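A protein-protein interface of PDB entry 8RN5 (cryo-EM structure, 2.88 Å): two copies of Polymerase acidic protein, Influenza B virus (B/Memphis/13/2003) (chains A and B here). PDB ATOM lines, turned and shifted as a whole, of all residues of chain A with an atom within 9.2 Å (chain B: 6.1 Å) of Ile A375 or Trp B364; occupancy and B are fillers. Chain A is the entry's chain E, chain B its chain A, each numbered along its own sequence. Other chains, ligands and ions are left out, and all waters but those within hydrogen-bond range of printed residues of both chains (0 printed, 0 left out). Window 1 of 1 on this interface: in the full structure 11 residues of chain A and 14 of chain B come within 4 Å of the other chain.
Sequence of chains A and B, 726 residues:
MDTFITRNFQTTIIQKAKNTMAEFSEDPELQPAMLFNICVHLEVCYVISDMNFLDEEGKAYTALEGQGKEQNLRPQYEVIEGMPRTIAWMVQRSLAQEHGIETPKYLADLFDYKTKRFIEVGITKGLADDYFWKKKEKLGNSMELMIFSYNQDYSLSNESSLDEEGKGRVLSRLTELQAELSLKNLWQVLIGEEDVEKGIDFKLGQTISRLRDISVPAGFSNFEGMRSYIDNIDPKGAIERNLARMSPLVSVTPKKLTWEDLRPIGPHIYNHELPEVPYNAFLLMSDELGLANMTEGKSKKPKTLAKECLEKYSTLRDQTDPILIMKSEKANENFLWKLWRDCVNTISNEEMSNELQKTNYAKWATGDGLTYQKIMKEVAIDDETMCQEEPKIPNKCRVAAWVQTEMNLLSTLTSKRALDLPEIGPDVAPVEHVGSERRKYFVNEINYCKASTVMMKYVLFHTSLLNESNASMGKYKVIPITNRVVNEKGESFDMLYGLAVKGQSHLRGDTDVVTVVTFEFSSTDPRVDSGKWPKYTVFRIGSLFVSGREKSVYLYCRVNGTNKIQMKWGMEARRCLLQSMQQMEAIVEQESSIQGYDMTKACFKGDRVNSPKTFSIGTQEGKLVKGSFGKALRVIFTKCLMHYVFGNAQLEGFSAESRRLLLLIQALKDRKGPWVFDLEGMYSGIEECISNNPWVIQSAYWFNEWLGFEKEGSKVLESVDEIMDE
The side-chain hydroxyl of Tyr B361 sits close to the side-chain carboxylate of Asp A382 (2.3 Å).
O of Lys B363 lies within hydrogen-bond range of N of Asp B368 (3.1 Å).
The backbone carbonyl oxygen of Lys B363 lies within hydrogen-bond range of the backbone NH of Gly B369 (3.1 Å).
NE2 of Gln A373 touches NZ of Lys B363, 3.8 Å away.
CZ2 of Trp B364 touches NE2 of Gln A373, 3.7 Å away.
CG2 of Ile A375 touches CZ2 of Trp B364, at 3.3 Å.
Asn B360 touches Met A376.
Met A376 touches Tyr B361 (SD to N, 3.98 Å).
Glu A378 touches Tyr B361.
CG1 of Val A379 touches CZ of Phe B335 (3.7 Å).
Tyr B361 touches Val A379 (CD2 to CG2, 3.8 Å).
Val A379 touches Trp B364.
Asp A382 touches Phe B335.
Of the printed residues of chain B, Ile A375 touches Trp B364 (3.3 Å).
Printed residues of chain B within 4 Å of Met A376: Asn B360 (3.8 Å) and Tyr B361 (3.98 Å).
Of the printed residues of chain A, Phe B335 touches Val A379 (3.7 Å) and Asp A382 (3.5 Å).
Of the printed residues of chain A, Asn B360 touches Met A376.
Printed residues of chain A within 4 Å of Tyr B361: Met A376 (3.98 Å), Glu A378 (3.4 Å), Val A379 (3.8 Å) and Asp A382 (2.3 Å).
Lys B363 touches just one residue of chain A: Gln A373.
Printed residues of chain A within 4 Å of Trp B364: Gln A373 (3.7 Å), Ile A375 (3.3 Å) and Val A379 (3.6 Å).
No residue of chain A comes within 4 Å of Gly B369.
The nearest printed residue of chain A that does not touch Trp B364 is Met A376 (5.2 Å).
The nearest printed residue of chain B that does not touch Asp A382 is Ala B365 (7.9 Å).
Hydrophobic or aromatic side chains of chain B that line the printed part of chain A: Phe B335, Tyr B361 and Trp B364.
Of the 13 printed residues of chain A, 6 touch a printed residue of chain B.
Along chain A the printed residues that touch a printed residue of chain B span positions 373 to 382.
Among the printed residues, no Asp or Glu carboxylate lies within 4 Å of a Lys or Arg side-chain nitrogen of the other chain.
No position is printed for both chains.
Of the 11 pairs that touch across the chains among the printed residues, none has its exchanged pair printed and touching as well.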
ATOM      1  N   TYR A 372     -17.062 -15.524   4.768  1.00  0.00           N
ATOM      2  CA  TYR A 372     -16.689 -15.900   3.413  1.00  0.00           C
ATOM      3  C   TYR A 372     -17.927 -16.085   2.546  1.00  0.00           C
ATOM      4  O   TYR A 372     -18.920 -16.683   2.968  1.00  0.00           O
ATOM      5  CB  TYR A 372     -15.867 -17.187   3.436  1.00  0.00           C
ATOM      6  CG  TYR A 372     -14.432 -17.003   3.878  1.00  0.00           C
ATOM      7  CD1 TYR A 372     -14.035 -15.879   4.590  1.00  0.00           C
ATOM      8  CD2 TYR A 372     -13.474 -17.958   3.588  1.00  0.00           C
ATOM      9  CE1 TYR A 372     -12.728 -15.715   4.993  1.00  0.00           C
ATOM     10  CE2 TYR A 372     -12.164 -17.802   3.987  1.00  0.00           C
ATOM     11  CZ  TYR A 372     -11.796 -16.679   4.689  1.00  0.00           C
ATOM     12  OH  TYR A 372     -10.489 -16.520   5.089  1.00  0.00           O
ATOM     13  N   GLN A 373     -17.861 -15.569   1.321  1.00  0.00           N
ATOM     14  CA  GLN A 373     -18.980 -15.668   0.396  1.00  0.00           C
ATOM     15  C   GLN A 373     -19.065 -17.068  -0.197  1.00  0.00           C
ATOM     16  O   GLN A 373     -18.050 -17.681  -0.533  1.00  0.00           O
ATOM     17  CB  GLN A 373     -18.839 -14.639  -0.725  1.00  0.00           C
ATOM     18  CG  GLN A 373     -19.980 -14.668  -1.726  1.00  0.00           C
ATOM     19  CD  GLN A 373     -19.988 -13.461  -2.636  1.00  0.00           C
ATOM     20  OE1 GLN A 373     -19.151 -12.567  -2.509  1.00  0.00           O
ATOM     21  NE2 GLN A 373     -20.938 -13.426  -3.562  1.00  0.00           N
ATOM     22  N   LYS A 374     -20.291 -17.567  -0.325  1.00  0.00           N
ATOM     23  CA  LYS A 374     -20.539 -18.871  -0.920  1.00  0.00           C
ATOM     24  C   LYS A 374     -20.735 -18.724  -2.423  1.00  0.00           C
ATOM     25  O   LYS A 374     -21.441 -17.822  -2.882  1.00  0.00           O
ATOM     26  CB  LYS A 374     -21.767 -19.525  -0.290  1.00  0.00           C
ATOM     27  CG  LYS A 374     -21.940 -20.990  -0.648  1.00  0.00           C
ATOM     28  CD  LYS A 374     -22.160 -21.846   0.589  1.00  0.00           C
ATOM     29  CE  LYS A 374     -22.530 -23.272   0.218  1.00  0.00           C
ATOM     30  NZ  LYS A 374     -23.077 -24.030   1.377  1.00  0.00           N
ATOM     31  N   ILE A 375     -20.102 -19.614  -3.187  1.00  0.00           N
ATOM     32  CA  ILE A 375     -20.169 -19.585  -4.641  1.00  0.00           C
ATOM     33  C   ILE A 375     -20.574 -20.962  -5.146  1.00  0.00           C
ATOM     34  O   ILE A 375     -20.396 -21.979  -4.473  1.00  0.00           O
ATOM     35  CB  ILE A 375     -18.834 -19.144  -5.281  1.00  0.00           C
ATOM     36  CG1 ILE A 375     -17.726 -20.160  -4.992  1.00  0.00           C
ATOM     37  CG2 ILE A 375     -18.434 -17.774  -4.766  1.00  0.00           C
ATOM     38  CD1 ILE A 375     -16.414 -19.826  -5.663  1.00  0.00           C
ATOM     39  N   MET A 376     -21.127 -20.979  -6.356  1.00  0.00           N
ATOM     40  CA  MET A 376     -21.604 -22.226  -6.941  1.00  0.00           C
ATOM     41  C   MET A 376     -20.445 -23.196  -7.134  1.00  0.00           C
ATOM     42  O   MET A 376     -19.320 -22.796  -7.447  1.00  0.00           O
ATOM     43  CB  MET A 376     -22.314 -21.967  -8.278  1.00  0.00           C
ATOM     44  CG  MET A 376     -21.835 -20.743  -9.064  1.00  0.00           C
ATOM     45  SD  MET A 376     -22.633 -20.523 -10.671  1.00  0.00           S
ATOM     46  CE  MET A 376     -22.500 -22.155 -11.390  1.00  0.00           C
ATOM     47  N   LYS A 377     -20.729 -24.487  -6.943  1.00  0.00           N
ATOM     48  CA  LYS A 377     -19.665 -25.485  -6.907  1.00  0.00           C
ATOM     49  C   LYS A 377     -18.889 -25.543  -8.216  1.00  0.00           C
ATOM     50  O   LYS A 377     -17.713 -25.922  -8.219  1.00  0.00           O
ATOM     51  CB  LYS A 377     -20.248 -26.860  -6.577  1.00  0.00           C
ATOM     52  CG  LYS A 377     -21.342 -27.322  -7.527  1.00  0.00           C
ATOM     53  CD  LYS A 377     -21.367 -28.835  -7.653  1.00  0.00           C
ATOM     54  CE  LYS A 377     -22.539 -29.306  -8.498  1.00  0.00           C
ATOM     55  NZ  LYS A 377     -22.540 -28.692  -9.854  1.00  0.00           N
ATOM     56  N   GLU A 378     -19.521 -25.187  -9.336  1.00  0.00           N
ATOM     57  CA  GLU A 378     -18.819 -25.208 -10.617  1.00  0.00           C
ATOM     58  C   GLU A 378     -17.631 -24.253 -10.600  1.00  0.00           C
ATOM     59  O   GLU A 378     -16.514 -24.619 -10.988  1.00  0.00           O
ATOM     60  CB  GLU A 378     -19.789 -24.845 -11.742  1.00  0.00           C
ATOM     61  CG  GLU A 378     -19.187 -24.860 -13.141  1.00  0.00           C
ATOM     62  CD  GLU A 378     -19.604 -26.072 -13.948  1.00  0.00           C
ATOM     63  OE1 GLU A 378     -19.864 -27.135 -13.344  1.00  0.00           O
ATOM     64  OE2 GLU A 378     -19.673 -25.962 -15.191  1.00  0.00           O
ATOM     65  N   VAL A 379     -17.856 -23.021 -10.140  1.00  0.00           N
ATOM     66  CA  VAL A 379     -16.785 -22.030 -10.104  1.00  0.00           C
ATOM     67  C   VAL A 379     -15.677 -22.481  -9.163  1.00  0.00           C
ATOM     68  O   VAL A 379     -14.487 -22.353  -9.474  1.00  0.00           O
ATOM     69  CB  VAL A 379     -17.351 -20.657  -9.697  1.00  0.00           C
ATOM     70  CG1 VAL A 379     -16.234 -19.639  -9.549  1.00  0.00           C
ATOM     71  CG2 VAL A 379     -18.375 -20.187 -10.716  1.00  0.00           C
ATOM     72  N   ALA A 380     -16.047 -23.007  -7.994  1.00  0.00           N
ATOM     73  CA  ALA A 380     -15.042 -23.450  -7.035  1.00  0.00           C
ATOM     74  C   ALA A 380     -14.207 -24.592  -7.597  1.00  0.00           C
ATOM     75  O   ALA A 380     -12.980 -24.609  -7.443  1.00  0.00           O
ATOM     76  CB  ALA A 380     -15.716 -23.870  -5.731  1.00  0.00           C
ATOM     77  N   ILE A 381     -14.851 -25.559  -8.251  1.00  0.00           N
ATOM     78  CA  ILE A 381     -14.113 -26.671  -8.841  1.00  0.00           C
ATOM     79  C   ILE A 381     -13.175 -26.164  -9.926  1.00  0.00           C
ATOM     80  O   ILE A 381     -12.015 -26.586 -10.012  1.00  0.00           O
ATOM     81  CB  ILE A 381     -15.087 -27.733  -9.383  1.00  0.00           C
ATOM     82  CG1 ILE A 381     -15.883 -28.364  -8.240  1.00  0.00           C
ATOM     83  CG2 ILE A 381     -14.331 -28.806 -10.150  1.00  0.00           C
ATOM     84  CD1 ILE A 381     -17.215 -28.932  -8.669  1.00  0.00           C
ATOM     85  N   ASP A 382     -13.658 -25.251 -10.772  1.00  0.00           N
ATOM     86  CA  ASP A 382     -12.815 -24.711 -11.832  1.00  0.00           C
ATOM     87  C   ASP A 382     -11.641 -23.912 -11.285  1.00  0.00           C
ATOM     88  O   ASP A 382     -10.648 -23.729 -11.997  1.00  0.00           O
ATOM     89  CB  ASP A 382     -13.645 -23.829 -12.763  1.00  0.00           C
ATOM     90  CG  ASP A 382     -14.422 -24.632 -13.785  1.00  0.00           C
ATOM     91  OD1 ASP A 382     -13.916 -25.683 -14.231  1.00  0.00           O
ATOM     92  OD2 ASP A 382     -15.538 -24.208 -14.147  1.00  0.00           O
ATOM     93  N   ASP A 383     -11.726 -23.436 -10.046  1.00  0.00           N
ATOM     94  CA  ASP A 383     -10.669 -22.633  -9.444  1.00  0.00           C
ATOM     95  C   ASP A 383      -9.720 -23.541  -8.672  1.00  0.00           C
ATOM     96  O   ASP A 383     -10.140 -24.240  -7.744  1.00  0.00           O
ATOM     97  CB  ASP A 383     -11.263 -21.569  -8.523  1.00  0.00           C
ATOM     98  CG  ASP A 383     -10.274 -20.472  -8.188  1.00  0.00           C
ATOM     99  OD1 ASP A 383      -9.114 -20.559  -8.640  1.00  0.00           O
ATOM    100  OD2 ASP A 383     -10.657 -19.525  -7.470  1.00  0.00           O
ATOM    101  N   MET A 386      -8.877 -22.718  -4.581  1.00  0.00           N
ATOM    102  CA  MET A 386      -9.712 -23.188  -3.485  1.00  0.00           C
ATOM    103  C   MET A 386      -9.273 -24.580  -3.051  1.00  0.00           C
ATOM    104  O   MET A 386      -9.055 -25.463  -3.886  1.00  0.00           O
ATOM    105  CB  MET A 386     -11.179 -23.202  -3.908  1.00  0.00           C
ATOM    106  CG  MET A 386     -11.682 -21.860  -4.421  1.00  0.00           C
ATOM    107  SD  MET A 386     -13.477 -21.668  -4.397  1.00  0.00           S
ATOM    108  CE  MET A 386     -13.869 -22.057  -2.694  1.00  0.00           C
ATOM    109  N   PHE B 335     -11.867 -20.788 -16.447  1.00  0.00           N
ATOM    110  CA  PHE B 335     -12.790 -19.659 -16.499  1.00  0.00           C
ATOM    111  C   PHE B 335     -12.879 -19.095 -17.909  1.00  0.00           C
ATOM    112  O   PHE B 335     -13.974 -18.916 -18.453  1.00  0.00           O
ATOM    113  CB  PHE B 335     -12.349 -18.562 -15.527  1.00  0.00           C
ATOM    114  CG  PHE B 335     -12.606 -18.873 -14.077  1.00  0.00           C
ATOM    115  CD1 PHE B 335     -13.163 -20.079 -13.684  1.00  0.00           C
ATOM    116  CD2 PHE B 335     -12.295 -17.942 -13.102  1.00  0.00           C
ATOM    117  CE1 PHE B 335     -13.396 -20.346 -12.352  1.00  0.00           C
ATOM    118  CE2 PHE B 335     -12.526 -18.207 -11.772  1.00  0.00           C
ATOM    119  CZ  PHE B 335     -13.077 -19.409 -11.396  1.00  0.00           C
ATOM    120  N   ASN B 360     -23.891 -16.111 -13.928  1.00  0.00           N
ATOM    121  CA  ASN B 360     -23.378 -16.415 -12.600  1.00  0.00           C
ATOM    122  C   ASN B 360     -21.980 -17.002 -12.646  1.00  0.00           C
ATOM    123  O   ASN B 360     -21.123 -16.608 -11.852  1.00  0.00           O
ATOM    124  CB  ASN B 360     -24.320 -17.389 -11.880  1.00  0.00           C
ATOM    125  CG  ASN B 360     -25.220 -16.696 -10.878  1.00  0.00           C
ATOM    126  OD1 ASN B 360     -24.773 -15.843 -10.111  1.00  0.00           O
ATOM    127  ND2 ASN B 360     -26.496 -17.061 -10.877  1.00  0.00           N
ATOM    128  N   TYR B 361     -21.729 -17.935 -13.563  1.00  0.00           N
ATOM    129  CA  TYR B 361     -20.358 -18.338 -13.842  1.00  0.00           C
ATOM    130  C   TYR B 361     -19.567 -17.178 -14.426  1.00  0.00           C
ATOM    131  O   TYR B 361     -18.402 -16.971 -14.073  1.00  0.00           O
ATOM    132  CB  TYR B 361     -20.348 -19.530 -14.796  1.00  0.00           C
ATOM    133  CG  TYR B 361     -19.010 -20.221 -14.891  1.00  0.00           C
ATOM    134  CD1 TYR B 361     -17.965 -19.656 -15.608  1.00  0.00           C
ATOM    135  CD2 TYR B 361     -18.790 -21.437 -14.266  1.00  0.00           C
ATOM    136  CE1 TYR B 361     -16.743 -20.279 -15.696  1.00  0.00           C
ATOM    137  CE2 TYR B 361     -17.570 -22.068 -14.350  1.00  0.00           C
ATOM    138  CZ  TYR B 361     -16.551 -21.486 -15.068  1.00  0.00           C
ATOM    139  OH  TYR B 361     -15.333 -22.112 -15.154  1.00  0.00           O
ATOM    140  N   ALA B 362     -20.188 -16.408 -15.322  1.00  0.00           N
ATOM    141  CA  ALA B 362     -19.523 -15.250 -15.906  1.00  0.00           C
ATOM    142  C   ALA B 362     -19.217 -14.181 -14.869  1.00  0.00           C
ATOM    143  O   ALA B 362     -18.339 -13.344 -15.099  1.00  0.00           O
ATOM    144  CB  ALA B 362     -20.387 -14.660 -17.020  1.00  0.00           C
ATOM    145  N   LYS B 363     -19.921 -14.184 -13.737  1.00  0.00           N
ATOM    146  CA  LYS B 363     -19.629 -13.216 -12.686  1.00  0.00           C
ATOM    147  C   LYS B 363     -18.225 -13.416 -12.135  1.00  0.00           C
ATOM    148  O   LYS B 363     -17.510 -12.443 -11.866  1.00  0.00           O
ATOM    149  CB  LYS B 363     -20.666 -13.328 -11.568  1.00  0.00           C
ATOM    150  CG  LYS B 363     -20.353 -12.492 -10.336  1.00  0.00           C
ATOM    151  CD  LYS B 363     -21.461 -12.599  -9.304  1.00  0.00           C
ATOM    152  CE  LYS B 363     -21.036 -12.009  -7.971  1.00  0.00           C
ATOM    153  NZ  LYS B 363     -22.082 -12.182  -6.927  1.00  0.00           N
ATOM    154  N   TRP B 364     -17.813 -14.668 -11.954  1.00  0.00           N
ATOM    155  CA  TRP B 364     -16.495 -14.969 -11.409  1.00  0.00           C
ATOM    156  C   TRP B 364     -15.454 -15.209 -12.489  1.00  0.00           C
ATOM    157  O   TRP B 364     -14.262 -14.990 -12.246  1.00  0.00           O
ATOM    158  CB  TRP B 364     -16.582 -16.192 -10.493  1.00  0.00           C
ATOM    159  CG  TRP B 364     -17.573 -16.011  -9.391  1.00  0.00           C
ATOM    160  CD1 TRP B 364     -18.856 -16.469  -9.360  1.00  0.00           C
ATOM    161  CD2 TRP B 364     -17.369 -15.308  -8.162  1.00  0.00           C
ATOM    162  NE1 TRP B 364     -19.463 -16.098  -8.187  1.00  0.00           N
ATOM    163  CE2 TRP B 364     -18.570 -15.384  -7.433  1.00  0.00           C
ATOM    164  CE3 TRP B 364     -16.286 -14.623  -7.606  1.00  0.00           C
ATOM    165  CZ2 TRP B 364     -18.718 -14.802  -6.179  1.00  0.00           C
ATOM    166  CZ3 TRP B 364     -16.434 -14.048  -6.360  1.00  0.00           C
ATOM    167  CH2 TRP B 364     -17.641 -14.140  -5.661  1.00  0.00           C
ATOM    168  N   ALA B 365     -15.873 -15.649 -13.676  1.00  0.00           N
ATOM    169  CA  ALA B 365     -14.925 -15.846 -14.766  1.00  0.00           C
ATOM    170  C   ALA B 365     -14.280 -14.529 -15.172  1.00  0.00           C
ATOM    171  O   ALA B 365     -13.074 -14.473 -15.436  1.00  0.00           O
ATOM    172  CB  ALA B 365     -15.628 -16.492 -15.958  1.00  0.00           C
ATOM    173  N   THR B 366     -15.068 -13.457 -15.226  1.00  0.00           N
ATOM    174  CA  THR B 366     -14.548 -12.137 -15.554  1.00  0.00           C
ATOM    175  C   THR B 366     -13.854 -11.466 -14.378  1.00  0.00           C
ATOM    176  O   THR B 366     -13.226 -10.420 -14.566  1.00  0.00           O
ATOM    177  CB  THR B 366     -15.679 -11.230 -16.047  1.00  0.00           C
ATOM    178  OG1 THR B 366     -16.572 -10.945 -14.964  1.00  0.00           O
ATOM    179  CG2 THR B 366     -16.450 -11.889 -17.177  1.00  0.00           C
ATOM    180  N   GLY B 367     -13.950 -12.035 -13.179  1.00  0.00           N
ATOM    181  CA  GLY B 367     -13.379 -11.414 -12.003  1.00  0.00           C
ATOM    182  C   GLY B 367     -14.232 -10.335 -11.382  1.00  0.00           C
ATOM    183  O   GLY B 367     -13.758  -9.638 -10.478  1.00  0.00           O
ATOM    184  N   ASP B 368     -15.475 -10.168 -11.838  1.00  0.00           N
ATOM    185  CA  ASP B 368     -16.344  -9.149 -11.261  1.00  0.00           C
ATOM    186  C   ASP B 368     -16.625  -9.433  -9.793  1.00  0.00           C
ATOM    187  O   ASP B 368     -16.646  -8.513  -8.967  1.00  0.00           O
ATOM    188  CB  ASP B 368     -17.651  -9.070 -12.048  1.00  0.00           C
ATOM    189  CG  ASP B 368     -17.482  -8.397 -13.395  1.00  0.00           C
ATOM    190  OD1 ASP B 368     -16.381  -7.874 -13.666  1.00  0.00           O
ATOM    191  OD2 ASP B 368     -18.450  -8.391 -14.182  1.00  0.00           O
ATOM    192  N   GLY B 369     -16.844 -10.701  -9.444  1.00  0.00           N
ATOM    193  CA  GLY B 369     -17.154 -11.048  -8.071  1.00  0.00           C
ATOM    194  C   GLY B 369     -16.031 -10.761  -7.099  1.00  0.00           C
ATOM    195  O   GLY B 369     -16.283 -10.627  -5.897  1.00  0.00           O
ATOM    196  N   LEU B 370     -14.795 -10.667  -7.585  1.00  0.00           N
ATOM    197  CA  LEU B 370     -13.645 -10.373  -6.732  1.00  0.00           C
ATOM    198  C   LEU B 370     -13.444  -8.862  -6.613  1.00  0.00           C
ATOM    199  O   LEU B 370     -12.431  -8.299  -7.024  1.00  0.00           O
ATOM    200  CB  LEU B 370     -12.394 -11.052  -7.278  1.00  0.00           C
ATOM    201  CG  LEU B 370     -12.287 -12.571  -7.140  1.00  0.00           C
ATOM    202  CD1 LEU B 370     -10.879 -13.021  -7.485  1.00  0.00           C
ATOM    203  CD2 LEU B 370     -12.665 -13.039  -5.746  1.00  0.00           C
ATOM    204  N   TYR B 476     -24.442  -9.481 -18.654  1.00  0.00           N
ATOM    205  CA  TYR B 476     -23.283  -9.827 -19.466  1.00  0.00           C
ATOM    206  C   TYR B 476     -23.722 -10.042 -20.906  1.00  0.00           C
ATOM    207  O   TYR B 476     -24.636 -10.828 -21.171  1.00  0.00           O
ATOM    208  CB  TYR B 476     -22.599 -11.078 -18.916  1.00  0.00           C
ATOM    209  CG  TYR B 476     -21.973 -10.851 -17.561  1.00  0.00           C
ATOM    210  CD1 TYR B 476     -22.753 -10.790 -16.417  1.00  0.00           C
ATOM    211  CD2 TYR B 476     -20.605 -10.691 -17.426  1.00  0.00           C
ATOM    212  CE1 TYR B 476     -22.189 -10.573 -15.181  1.00  0.00           C
ATOM    213  CE2 TYR B 476     -20.031 -10.471 -16.195  1.00  0.00           C
ATOM    214  CZ  TYR B 476     -20.826 -10.415 -15.076  1.00  0.00           C
ATOM    215  OH  TYR B 476     -20.256 -10.198 -13.844  1.00  0.00           O
